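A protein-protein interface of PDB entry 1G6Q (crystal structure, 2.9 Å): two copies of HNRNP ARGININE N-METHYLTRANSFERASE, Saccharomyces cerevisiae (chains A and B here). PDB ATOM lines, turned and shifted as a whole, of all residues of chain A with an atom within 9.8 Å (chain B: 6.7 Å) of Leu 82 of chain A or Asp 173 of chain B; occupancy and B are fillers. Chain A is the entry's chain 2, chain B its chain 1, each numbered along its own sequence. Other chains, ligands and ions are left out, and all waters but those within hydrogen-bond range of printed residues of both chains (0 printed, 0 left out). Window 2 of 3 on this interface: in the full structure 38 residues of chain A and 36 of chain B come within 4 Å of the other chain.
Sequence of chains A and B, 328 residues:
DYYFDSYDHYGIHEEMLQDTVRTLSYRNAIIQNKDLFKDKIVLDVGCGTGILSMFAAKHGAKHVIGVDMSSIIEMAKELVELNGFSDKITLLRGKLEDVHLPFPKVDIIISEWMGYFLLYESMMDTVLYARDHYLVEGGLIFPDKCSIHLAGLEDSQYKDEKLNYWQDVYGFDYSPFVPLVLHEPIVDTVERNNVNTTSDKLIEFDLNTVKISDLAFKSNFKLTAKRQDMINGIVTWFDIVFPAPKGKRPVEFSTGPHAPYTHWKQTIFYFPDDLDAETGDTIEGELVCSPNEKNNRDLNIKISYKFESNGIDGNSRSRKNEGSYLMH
The side-chain amide oxygen (OD1) of Asn 83 of chain A lies within hydrogen-bond range of the backbone NH (N) of Asp 173 of chain B, 2.7 Å away. OH of Tyr 174 of chain B is in hydrogen-bond range of OG1 of Thr 49 of chain A.
Of the printed residues of chain B, Lys 58 of chain A touches Phe 172 (3.9 Å). Of the printed residues of chain B, Leu 79 of chain A touches Asp 173 (3.95 Å), Tyr 174 (3.6 Å) and Pro 176 (3.6 Å). Leu 82 of chain A touches just these residues of chain B: Asp 173 and Pro 176. Of the printed residues of chain A, Phe 172 of chain B touches Ile 51, Met 54, Lys 58, Asn 83 and Phe 85. Asp 173 of chain B touches just these residues of chain A: Leu 79, Leu 82 and Asn 83. The nearest residue of chain B that does not touch Leu 82 of chain A is Ser 175 of chain B (4.6 Å). The nearest printed residue of chain A that does not touch Phe 172 of chain B is Leu 79 of chain A (6.6 Å).
The backbone carbonyl oxygen (O) of Trp 166 of chain B is in hydrogen-bond range of the backbone NH (N) of Tyr 174 of chain B (3.0 Å). The side-chain carboxylate (OD1) of Asp 173 of chain B is in hydrogen-bond range of the side-chain hydroxyl (OG) of Ser 175 of chain B (2.8 Å). The backbone carbonyl oxygen (O) of Leu 79 of chain A lies within hydrogen-bond range of the side-chain amide nitrogen (ND2) of Asn 83 of chain A (3.0 Å). The backbone NH (N) of Phe 85 of chain A sits at hydrogen-bond distance from the backbone carbonyl oxygen (O) of Val 80 of chain A, 2.7 Å away.
Of the 19 printed residues of chain A, 10 touch a printed residue of chain B. Hydrophobic or aromatic side chains of chain A within 4 Å of the printed part of chain B: Ile 51, Met 54, Met 75, Leu 79, Leu 82 and Phe 85. Of the 10 printed residues of chain B, 4 touch a printed residue of chain A.
Among the printed residues, pairs that only touch across the chains: Asn 83 of chain A with Phe 172 of chain B, Glu 78 of chain A with Pro 176 of chain B, Leu 82 of chain A with Asp 173 of chain B, Ile 51 of chain A with Tyr 174 of chain B, Phe 85 of chain A with Phe 172 of chain B, Leu 82 of chain A with Pro 176 of chain B, Leu 79 of chain A with Pro 176 of chain B, Leu 79 of chain A with Tyr 174 of chain B, Met 54 of chain A with Phe 172 of chain B, Met 75 of chain A with Pro 176 of chain B, Ile 51 of chain A with Phe 172 of chain B, Lys 58 of chain A with Phe 172 of chain B and Leu 79 of chain A with Asp 173 of chain B.
No position is printed for both chains. Of the 15 pairs that touch across the chains among the printed residues, none has its exchanged pair printed and touching as well.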
ATOM      1  N   THR A  49       5.641  14.438 -19.635  1.00  0.00           N
ATOM      2  CA  THR A  49       5.516  13.547 -20.785  1.00  0.00           C
ATOM      3  C   THR A  49       5.566  12.075 -20.386  1.00  0.00           C
ATOM      4  O   THR A  49       5.693  11.174 -21.219  1.00  0.00           O
ATOM      5  CB  THR A  49       6.637  13.838 -21.733  1.00  0.00           C
ATOM      6  OG1 THR A  49       7.888  13.594 -21.084  1.00  0.00           O
ATOM      7  CG2 THR A  49       6.585  15.284 -22.088  1.00  0.00           C
ATOM      8  N   ILE A  51       8.050  10.398 -19.172  1.00  0.00           N
ATOM      9  CA  ILE A  51       9.404   9.811 -19.156  1.00  0.00           C
ATOM     10  C   ILE A  51       9.756   9.014 -17.896  1.00  0.00           C
ATOM     11  O   ILE A  51      10.125   7.852 -18.021  1.00  0.00           O
ATOM     12  CB  ILE A  51      10.414  10.977 -19.384  1.00  0.00           C
ATOM     13  CG1 ILE A  51      11.833  10.484 -19.337  1.00  0.00           C
ATOM     14  CG2 ILE A  51      10.287  12.033 -18.275  1.00  0.00           C
ATOM     15  CD1 ILE A  51      12.238   9.520 -20.453  1.00  0.00           C
ATOM     16  N   MET A  54       7.786   5.802 -17.761  1.00  0.00           N
ATOM     17  CA  MET A  54       8.274   4.821 -18.691  1.00  0.00           C
ATOM     18  C   MET A  54       9.577   4.203 -18.213  1.00  0.00           C
ATOM     19  O   MET A  54       9.753   2.991 -18.345  1.00  0.00           O
ATOM     20  CB  MET A  54       8.434   5.467 -20.018  1.00  0.00           C
ATOM     21  CG  MET A  54       7.075   5.561 -20.682  1.00  0.00           C
ATOM     22  SD  MET A  54       7.246   6.102 -22.405  1.00  0.00           S
ATOM     23  CE  MET A  54       7.362   7.821 -22.023  1.00  0.00           C
ATOM     24  N   LYS A  58       9.772   0.337 -17.649  1.00  0.00           N
ATOM     25  CA  LYS A  58      10.845  -0.292 -18.413  1.00  0.00           C
ATOM     26  C   LYS A  58      11.659  -1.206 -17.485  1.00  0.00           C
ATOM     27  O   LYS A  58      12.015  -2.335 -17.831  1.00  0.00           O
ATOM     28  CB  LYS A  58      11.763   0.775 -19.024  1.00  0.00           C
ATOM     29  CG  LYS A  58      12.952   0.180 -19.754  1.00  0.00           C
ATOM     30  CD  LYS A  58      13.883   1.223 -20.369  1.00  0.00           C
ATOM     31  CE  LYS A  58      14.993   0.509 -21.104  1.00  0.00           C
ATOM     32  NZ  LYS A  58      15.709   1.447 -21.916  1.00  0.00           N
ATOM     33  N   GLU A  74      -2.210  14.110 -22.430  1.00  0.00           N
ATOM     34  CA  GLU A  74      -2.756  13.469 -23.630  1.00  0.00           C
ATOM     35  C   GLU A  74      -1.678  13.012 -24.630  1.00  0.00           C
ATOM     36  O   GLU A  74      -1.699  11.914 -25.203  1.00  0.00           O
ATOM     37  CB  GLU A  74      -3.755  14.439 -24.254  1.00  0.00           C
ATOM     38  CG  GLU A  74      -4.960  14.747 -23.333  1.00  0.00           C
ATOM     39  CD  GLU A  74      -5.670  13.537 -22.708  1.00  0.00           C
ATOM     40  OE1 GLU A  74      -6.142  12.651 -23.423  1.00  0.00           O
ATOM     41  OE2 GLU A  74      -5.756  13.487 -21.480  1.00  0.00           O
ATOM     42  N   MET A  75      -0.625  13.830 -24.706  1.00  0.00           N
ATOM     43  CA  MET A  75       0.582  13.477 -25.442  1.00  0.00           C
ATOM     44  C   MET A  75       1.230  12.233 -24.804  1.00  0.00           C
ATOM     45  O   MET A  75       1.382  11.179 -25.412  1.00  0.00           O
ATOM     46  CB  MET A  75       1.492  14.687 -25.394  1.00  0.00           C
ATOM     47  CG  MET A  75       2.887  14.403 -25.935  1.00  0.00           C
ATOM     48  SD  MET A  75       2.833  13.626 -27.602  1.00  0.00           S
ATOM     49  CE  MET A  75       2.909  15.202 -28.382  1.00  0.00           C
ATOM     50  N   ALA A  76       1.505  12.304 -23.507  1.00  0.00           N
ATOM     51  CA  ALA A  76       2.123  11.213 -22.771  1.00  0.00           C
ATOM     52  C   ALA A  76       1.335   9.924 -22.878  1.00  0.00           C
ATOM     53  O   ALA A  76       1.899   8.832 -22.899  1.00  0.00           O
ATOM     54  CB  ALA A  76       2.268  11.577 -21.300  1.00  0.00           C
ATOM     55  N   LYS A  77       0.028   9.998 -23.081  1.00  0.00           N
ATOM     56  CA  LYS A  77      -0.717   8.757 -23.315  1.00  0.00           C
ATOM     57  C   LYS A  77      -0.292   8.197 -24.656  1.00  0.00           C
ATOM     58  O   LYS A  77       0.146   7.051 -24.728  1.00  0.00           O
ATOM     59  CB  LYS A  77      -2.189   8.995 -23.336  1.00  0.00           C
ATOM     60  CG  LYS A  77      -2.582   9.324 -21.919  1.00  0.00           C
ATOM     61  CD  LYS A  77      -4.067   9.534 -21.973  1.00  0.00           C
ATOM     62  CE  LYS A  77      -4.665   9.653 -20.594  1.00  0.00           C
ATOM     63  NZ  LYS A  77      -6.098   9.433 -20.723  1.00  0.00           N
ATOM     64  N   GLU A  78      -0.216   9.035 -25.704  1.00  0.00           N
ATOM     65  CA  GLU A  78       0.274   8.587 -27.008  1.00  0.00           C
ATOM     66  C   GLU A  78       1.687   8.013 -26.931  1.00  0.00           C
ATOM     67  O   GLU A  78       2.016   6.987 -27.517  1.00  0.00           O
ATOM     68  CB  GLU A  78       0.266   9.751 -27.955  1.00  0.00           C
ATOM     69  CG  GLU A  78       0.198   9.186 -29.351  1.00  0.00           C
ATOM     70  CD  GLU A  78      -0.085  10.199 -30.439  1.00  0.00           C
ATOM     71  OE1 GLU A  78       0.660  10.210 -31.417  1.00  0.00           O
ATOM     72  OE2 GLU A  78      -1.039  10.967 -30.323  1.00  0.00           O
ATOM     73  N   LEU A  79       2.528   8.613 -26.106  1.00  0.00           N
ATOM     74  CA  LEU A  79       3.890   8.128 -25.971  1.00  0.00           C
ATOM     75  C   LEU A  79       3.959   6.771 -25.274  1.00  0.00           C
ATOM     76  O   LEU A  79       4.688   5.851 -25.668  1.00  0.00           O
ATOM     77  CB  LEU A  79       4.669   9.158 -25.213  1.00  0.00           C
ATOM     78  CG  LEU A  79       4.946  10.465 -25.897  1.00  0.00           C
ATOM     79  CD1 LEU A  79       5.513  11.378 -24.888  1.00  0.00           C
ATOM     80  CD2 LEU A  79       5.957  10.362 -26.960  1.00  0.00           C
ATOM     81  N   VAL A  80       3.120   6.589 -24.255  1.00  0.00           N
ATOM     82  CA  VAL A  80       3.068   5.345 -23.499  1.00  0.00           C
ATOM     83  C   VAL A  80       2.495   4.201 -24.322  1.00  0.00           C
ATOM     84  O   VAL A  80       2.844   3.030 -24.127  1.00  0.00           O
ATOM     85  CB  VAL A  80       2.260   5.666 -22.252  1.00  0.00           C
ATOM     86  CG1 VAL A  80       1.654   4.453 -21.599  1.00  0.00           C
ATOM     87  CG2 VAL A  80       3.236   6.368 -21.318  1.00  0.00           C
ATOM     88  N   GLU A  81       1.607   4.487 -25.282  1.00  0.00           N
ATOM     89  CA  GLU A  81       1.186   3.433 -26.210  1.00  0.00           C
ATOM     90  C   GLU A  81       2.282   3.155 -27.247  1.00  0.00           C
ATOM     91  O   GLU A  81       2.704   2.017 -27.449  1.00  0.00           O
ATOM     92  CB  GLU A  81      -0.064   3.817 -26.973  1.00  0.00           C
ATOM     93  CG  GLU A  81      -1.150   2.730 -27.115  1.00  0.00           C
ATOM     94  CD  GLU A  81      -0.754   1.515 -27.933  1.00  0.00           C
ATOM     95  OE1 GLU A  81      -0.685   0.420 -27.360  1.00  0.00           O
ATOM     96  OE2 GLU A  81      -0.540   1.677 -29.137  1.00  0.00           O
ATOM     97  N   LEU A  82       2.850   4.187 -27.866  1.00  0.00           N
ATOM     98  CA  LEU A  82       3.899   3.974 -28.851  1.00  0.00           C
ATOM     99  C   LEU A  82       5.049   3.131 -28.328  1.00  0.00           C
ATOM    100  O   LEU A  82       5.529   2.263 -29.056  1.00  0.00           O
ATOM    101  CB  LEU A  82       4.454   5.314 -29.338  1.00  0.00           C
ATOM    102  CG  LEU A  82       5.443   5.220 -30.493  1.00  0.00           C
ATOM    103  CD1 LEU A  82       4.834   4.426 -31.646  1.00  0.00           C
ATOM    104  CD2 LEU A  82       5.812   6.621 -30.933  1.00  0.00           C
ATOM    105  N   ASN A  83       5.471   3.339 -27.067  1.00  0.00           N
ATOM    106  CA  ASN A  83       6.574   2.553 -26.541  1.00  0.00           C
ATOM    107  C   ASN A  83       6.136   1.275 -25.837  1.00  0.00           C
ATOM    108  O   ASN A  83       6.819   0.644 -25.022  1.00  0.00           O
ATOM    109  CB  ASN A  83       7.385   3.419 -25.613  1.00  0.00           C
ATOM    110  CG  ASN A  83       8.136   4.451 -26.407  1.00  0.00           C
ATOM    111  OD1 ASN A  83       9.283   4.275 -26.819  1.00  0.00           O
ATOM    112  ND2 ASN A  83       7.523   5.580 -26.704  1.00  0.00           N
ATOM    113  N   GLY A  84       4.925   0.872 -26.127  1.00  0.00           N
ATOM    114  CA  GLY A  84       4.461  -0.412 -25.624  1.00  0.00           C
ATOM    115  C   GLY A  84       4.137  -0.509 -24.146  1.00  0.00           C
ATOM    116  O   GLY A  84       4.045  -1.609 -23.613  1.00  0.00           O
ATOM    117  N   PHE A  85       3.886   0.585 -23.439  1.00  0.00           N
ATOM    118  CA  PHE A  85       3.572   0.472 -22.022  1.00  0.00           C
ATOM    119  C   PHE A  85       2.103   0.656 -21.660  1.00  0.00           C
ATOM    120  O   PHE A  85       1.727   0.619 -20.487  1.00  0.00           O
ATOM    121  CB  PHE A  85       4.429   1.487 -21.232  1.00  0.00           C
ATOM    122  CG  PHE A  85       5.916   1.187 -21.250  1.00  0.00           C
ATOM    123  CD1 PHE A  85       6.392   0.057 -20.609  1.00  0.00           C
ATOM    124  CD2 PHE A  85       6.784   2.020 -21.955  1.00  0.00           C
ATOM    125  CE1 PHE A  85       7.748  -0.236 -20.685  1.00  0.00           C
ATOM    126  CE2 PHE A  85       8.141   1.716 -22.024  1.00  0.00           C
ATOM    127  CZ  PHE A  85       8.624   0.586 -21.388  1.00  0.00           C
ATOM    128  N   SER A  86       1.200   0.842 -22.608  1.00  0.00           N
ATOM    129  CA  SER A  86      -0.221   1.105 -22.317  1.00  0.00           C
ATOM    130  C   SER A  86      -0.923   0.275 -21.261  1.00  0.00           C
ATOM    131  O   SER A  86      -1.824   0.720 -20.560  1.00  0.00           O
ATOM    132  CB  SER A  86      -1.043   0.997 -23.585  1.00  0.00           C
ATOM    133  OG  SER A  86      -0.580  -0.092 -24.379  1.00  0.00           O
ATOM    134  N   ASP A  87      -0.489  -0.958 -21.112  1.00  0.00           N
ATOM    135  CA  ASP A  87      -1.008  -1.862 -20.083  1.00  0.00           C
ATOM    136  C   ASP A  87      -0.473  -1.597 -18.666  1.00  0.00           C
ATOM    137  O   ASP A  87      -1.166  -1.702 -17.655  1.00  0.00           O
ATOM    138  CB  ASP A  87      -0.666  -3.294 -20.493  1.00  0.00           C
ATOM    139  CG  ASP A  87       0.843  -3.586 -20.559  1.00  0.00           C
ATOM    140  OD1 ASP A  87       1.543  -2.998 -21.395  1.00  0.00           O
ATOM    141  OD2 ASP A  87       1.313  -4.384 -19.742  1.00  0.00           O
ATOM    142  N   ILE A  89       1.041   1.454 -17.628  1.00  0.00           N
ATOM    143  CA  ILE A  89       0.961   2.836 -17.153  1.00  0.00           C
ATOM    144  C   ILE A  89      -0.400   3.495 -17.360  1.00  0.00           C
ATOM    145  O   ILE A  89      -0.992   3.506 -18.442  1.00  0.00           O
ATOM    146  CB  ILE A  89       1.988   3.772 -17.836  1.00  0.00           C
ATOM    147  CG1 ILE A  89       3.345   3.158 -17.859  1.00  0.00           C
ATOM    148  CG2 ILE A  89       2.057   5.108 -17.042  1.00  0.00           C
ATOM    149  CD1 ILE A  89       4.421   3.988 -18.553  1.00  0.00           C
ATOM    150  N   TRP B 166      13.502  14.429 -31.041  1.00  0.00           N
ATOM    151  CA  TRP B 166      12.424  13.549 -30.608  1.00  0.00           C
ATOM    152  C   TRP B 166      12.432  12.112 -31.104  1.00  0.00           C
ATOM    153  O   TRP B 166      11.675  11.248 -30.643  1.00  0.00           O
ATOM    154  CB  TRP B 166      11.123  14.214 -30.958  1.00  0.00           C
ATOM    155  CG  TRP B 166      11.139  15.583 -30.309  1.00  0.00           C
ATOM    156  CD1 TRP B 166      11.265  16.718 -31.063  1.00  0.00           C
ATOM    157  CD2 TRP B 166      11.011  15.851 -28.975  1.00  0.00           C
ATOM    158  NE1 TRP B 166      11.208  17.707 -30.224  1.00  0.00           N
ATOM    159  CE2 TRP B 166      11.062  17.250 -28.982  1.00  0.00           C
ATOM    160  CE3 TRP B 166      10.859  15.174 -27.785  1.00  0.00           C
ATOM    161  CZ2 TRP B 166      10.957  18.007 -27.815  1.00  0.00           C
ATOM    162  CZ3 TRP B 166      10.750  15.917 -26.613  1.00  0.00           C
ATOM    163  CH2 TRP B 166      10.798  17.321 -26.620  1.00  0.00           C
ATOM    164  N   GLN B 167      13.344  11.752 -31.995  1.00  0.00           N
ATOM    165  CA  GLN B 167      13.382  10.378 -32.474  1.00  0.00           C
ATOM    166  C   GLN B 167      13.873   9.410 -31.403  1.00  0.00           C
ATOM    167  O   GLN B 167      13.413   8.280 -31.353  1.00  0.00           O
ATOM    168  CB  GLN B 167      14.266  10.338 -33.697  1.00  0.00           C
ATOM    169  CG  GLN B 167      13.667  11.039 -34.912  1.00  0.00           C
ATOM    170  CD  GLN B 167      12.587  10.257 -35.669  1.00  0.00           C
ATOM    171  OE1 GLN B 167      11.393  10.492 -35.545  1.00  0.00           O
ATOM    172  NE2 GLN B 167      12.858   9.291 -36.523  1.00  0.00           N
ATOM    173  N   ASP B 168      14.779   9.784 -30.501  1.00  0.00           N
ATOM    174  CA  ASP B 168      15.121   8.900 -29.400  1.00  0.00           C
ATOM    175  C   ASP B 168      15.339   9.673 -28.125  1.00  0.00           C
ATOM    176  O   ASP B 168      16.401  10.291 -27.971  1.00  0.00           O
ATOM    177  CB  ASP B 168      16.372   8.146 -29.744  1.00  0.00           C
ATOM    178  CG  ASP B 168      16.858   7.167 -28.678  1.00  0.00           C
ATOM    179  OD1 ASP B 168      17.683   7.540 -27.844  1.00  0.00           O
ATOM    180  OD2 ASP B 168      16.408   6.021 -28.647  1.00  0.00           O
ATOM    181  N   VAL B 169      14.404   9.646 -27.185  1.00  0.00           N
ATOM    182  CA  VAL B 169      14.643  10.318 -25.928  1.00  0.00           C
ATOM    183  C   VAL B 169      15.007   9.243 -24.929  1.00  0.00           C
ATOM    184  O   VAL B 169      14.179   8.431 -24.565  1.00  0.00           O
ATOM    185  CB  VAL B 169      13.388  11.108 -25.502  1.00  0.00           C
ATOM    186  CG1 VAL B 169      13.611  11.825 -24.165  1.00  0.00           C
ATOM    187  CG2 VAL B 169      13.147  12.222 -26.509  1.00  0.00           C
ATOM    188  N   GLY B 171      16.270   6.310 -25.165  1.00  0.00           N
ATOM    189  CA  GLY B 171      15.746   4.993 -25.539  1.00  0.00           C
ATOM    190  C   GLY B 171      14.317   4.987 -26.055  1.00  0.00           C
ATOM    191  O   GLY B 171      13.982   4.250 -26.976  1.00  0.00           O
ATOM    192  N   PHE B 172      13.452   5.816 -25.511  1.00  0.00           N
ATOM    193  CA  PHE B 172      12.059   5.864 -25.940  1.00  0.00           C
ATOM    194  C   PHE B 172      11.819   6.545 -27.250  1.00  0.00           C
ATOM    195  O   PHE B 172      12.471   7.569 -27.501  1.00  0.00           O
ATOM    196  CB  PHE B 172      11.255   6.587 -24.934  1.00  0.00           C
ATOM    197  CG  PHE B 172      11.393   5.783 -23.697  1.00  0.00           C
ATOM    198  CD1 PHE B 172      12.054   6.300 -22.584  1.00  0.00           C
ATOM    199  CD2 PHE B 172      10.859   4.498 -23.717  1.00  0.00           C
ATOM    200  CE1 PHE B 172      12.171   5.503 -21.473  1.00  0.00           C
ATOM    201  CE2 PHE B 172      10.990   3.717 -22.595  1.00  0.00           C
ATOM    202  CZ  PHE B 172      11.638   4.214 -21.483  1.00  0.00           C
ATOM    203  N   ASP B 173      10.920   6.064 -28.104  1.00  0.00           N
ATOM    204  CA  ASP B 173      10.574   6.806 -29.308  1.00  0.00           C
ATOM    205  C   ASP B 173       9.661   7.978 -28.938  1.00  0.00           C
ATOM    206  O   ASP B 173       8.576   7.775 -28.400  1.00  0.00           O
ATOM    207  CB  ASP B 173       9.868   5.875 -30.274  1.00  0.00           C
ATOM    208  CG  ASP B 173       9.359   6.427 -31.611  1.00  0.00           C
ATOM    209  OD1 ASP B 173       9.601   7.583 -31.925  1.00  0.00           O
ATOM    210  OD2 ASP B 173       8.702   5.679 -32.346  1.00  0.00           O
ATOM    211  N   TYR B 174      10.068   9.220 -29.203  1.00  0.00           N
ATOM    212  CA  TYR B 174       9.220  10.375 -28.925  1.00  0.00           C
ATOM    213  C   TYR B 174       8.682  11.086 -30.170  1.00  0.00           C
ATOM    214  O   TYR B 174       8.146  12.205 -30.150  1.00  0.00           O
ATOM    215  CB  TYR B 174      10.009  11.319 -28.075  1.00  0.00           C
ATOM    216  CG  TYR B 174       9.702  11.264 -26.596  1.00  0.00           C
ATOM    217  CD1 TYR B 174       9.945  10.157 -25.785  1.00  0.00           C
ATOM    218  CD2 TYR B 174       9.210  12.436 -26.038  1.00  0.00           C
ATOM    219  CE1 TYR B 174       9.704  10.249 -24.413  1.00  0.00           C
ATOM    220  CE2 TYR B 174       8.968  12.530 -24.685  1.00  0.00           C
ATOM    221  CZ  TYR B 174       9.217  11.433 -23.876  1.00  0.00           C
ATOM    222  OH  TYR B 174       8.983  11.545 -22.515  1.00  0.00           O
ATOM    223  N   SER B 175       8.686  10.385 -31.313  1.00  0.00           N
ATOM    224  CA  SER B 175       8.121  10.866 -32.581  1.00  0.00           C
ATOM    225  C   SER B 175       6.805  11.597 -32.554  1.00  0.00           C
ATOM    226  O   SER B 175       6.625  12.477 -33.396  1.00  0.00           O
ATOM    227  CB  SER B 175       7.865   9.780 -33.586  1.00  0.00           C
ATOM    228  OG  SER B 175       9.044   9.259 -34.161  1.00  0.00           O
ATOM    229  N   PRO B 176       5.804  11.342 -31.720  1.00  0.00           N
ATOM    230  CA  PRO B 176       4.602  12.139 -31.766  1.00  0.00           C
ATOM    231  C   PRO B 176       4.868  13.600 -31.451  1.00  0.00           C
ATOM    232  O   PRO B 176       4.086  14.449 -31.854  1.00  0.00           O
ATOM    233  CB  PRO B 176       3.672  11.490 -30.801  1.00  0.00           C
ATOM    234  CG  PRO B 176       4.348  10.272 -30.231  1.00  0.00           C
ATOM    235  CD  PRO B 176       5.710  10.194 -30.838  1.00  0.00           C
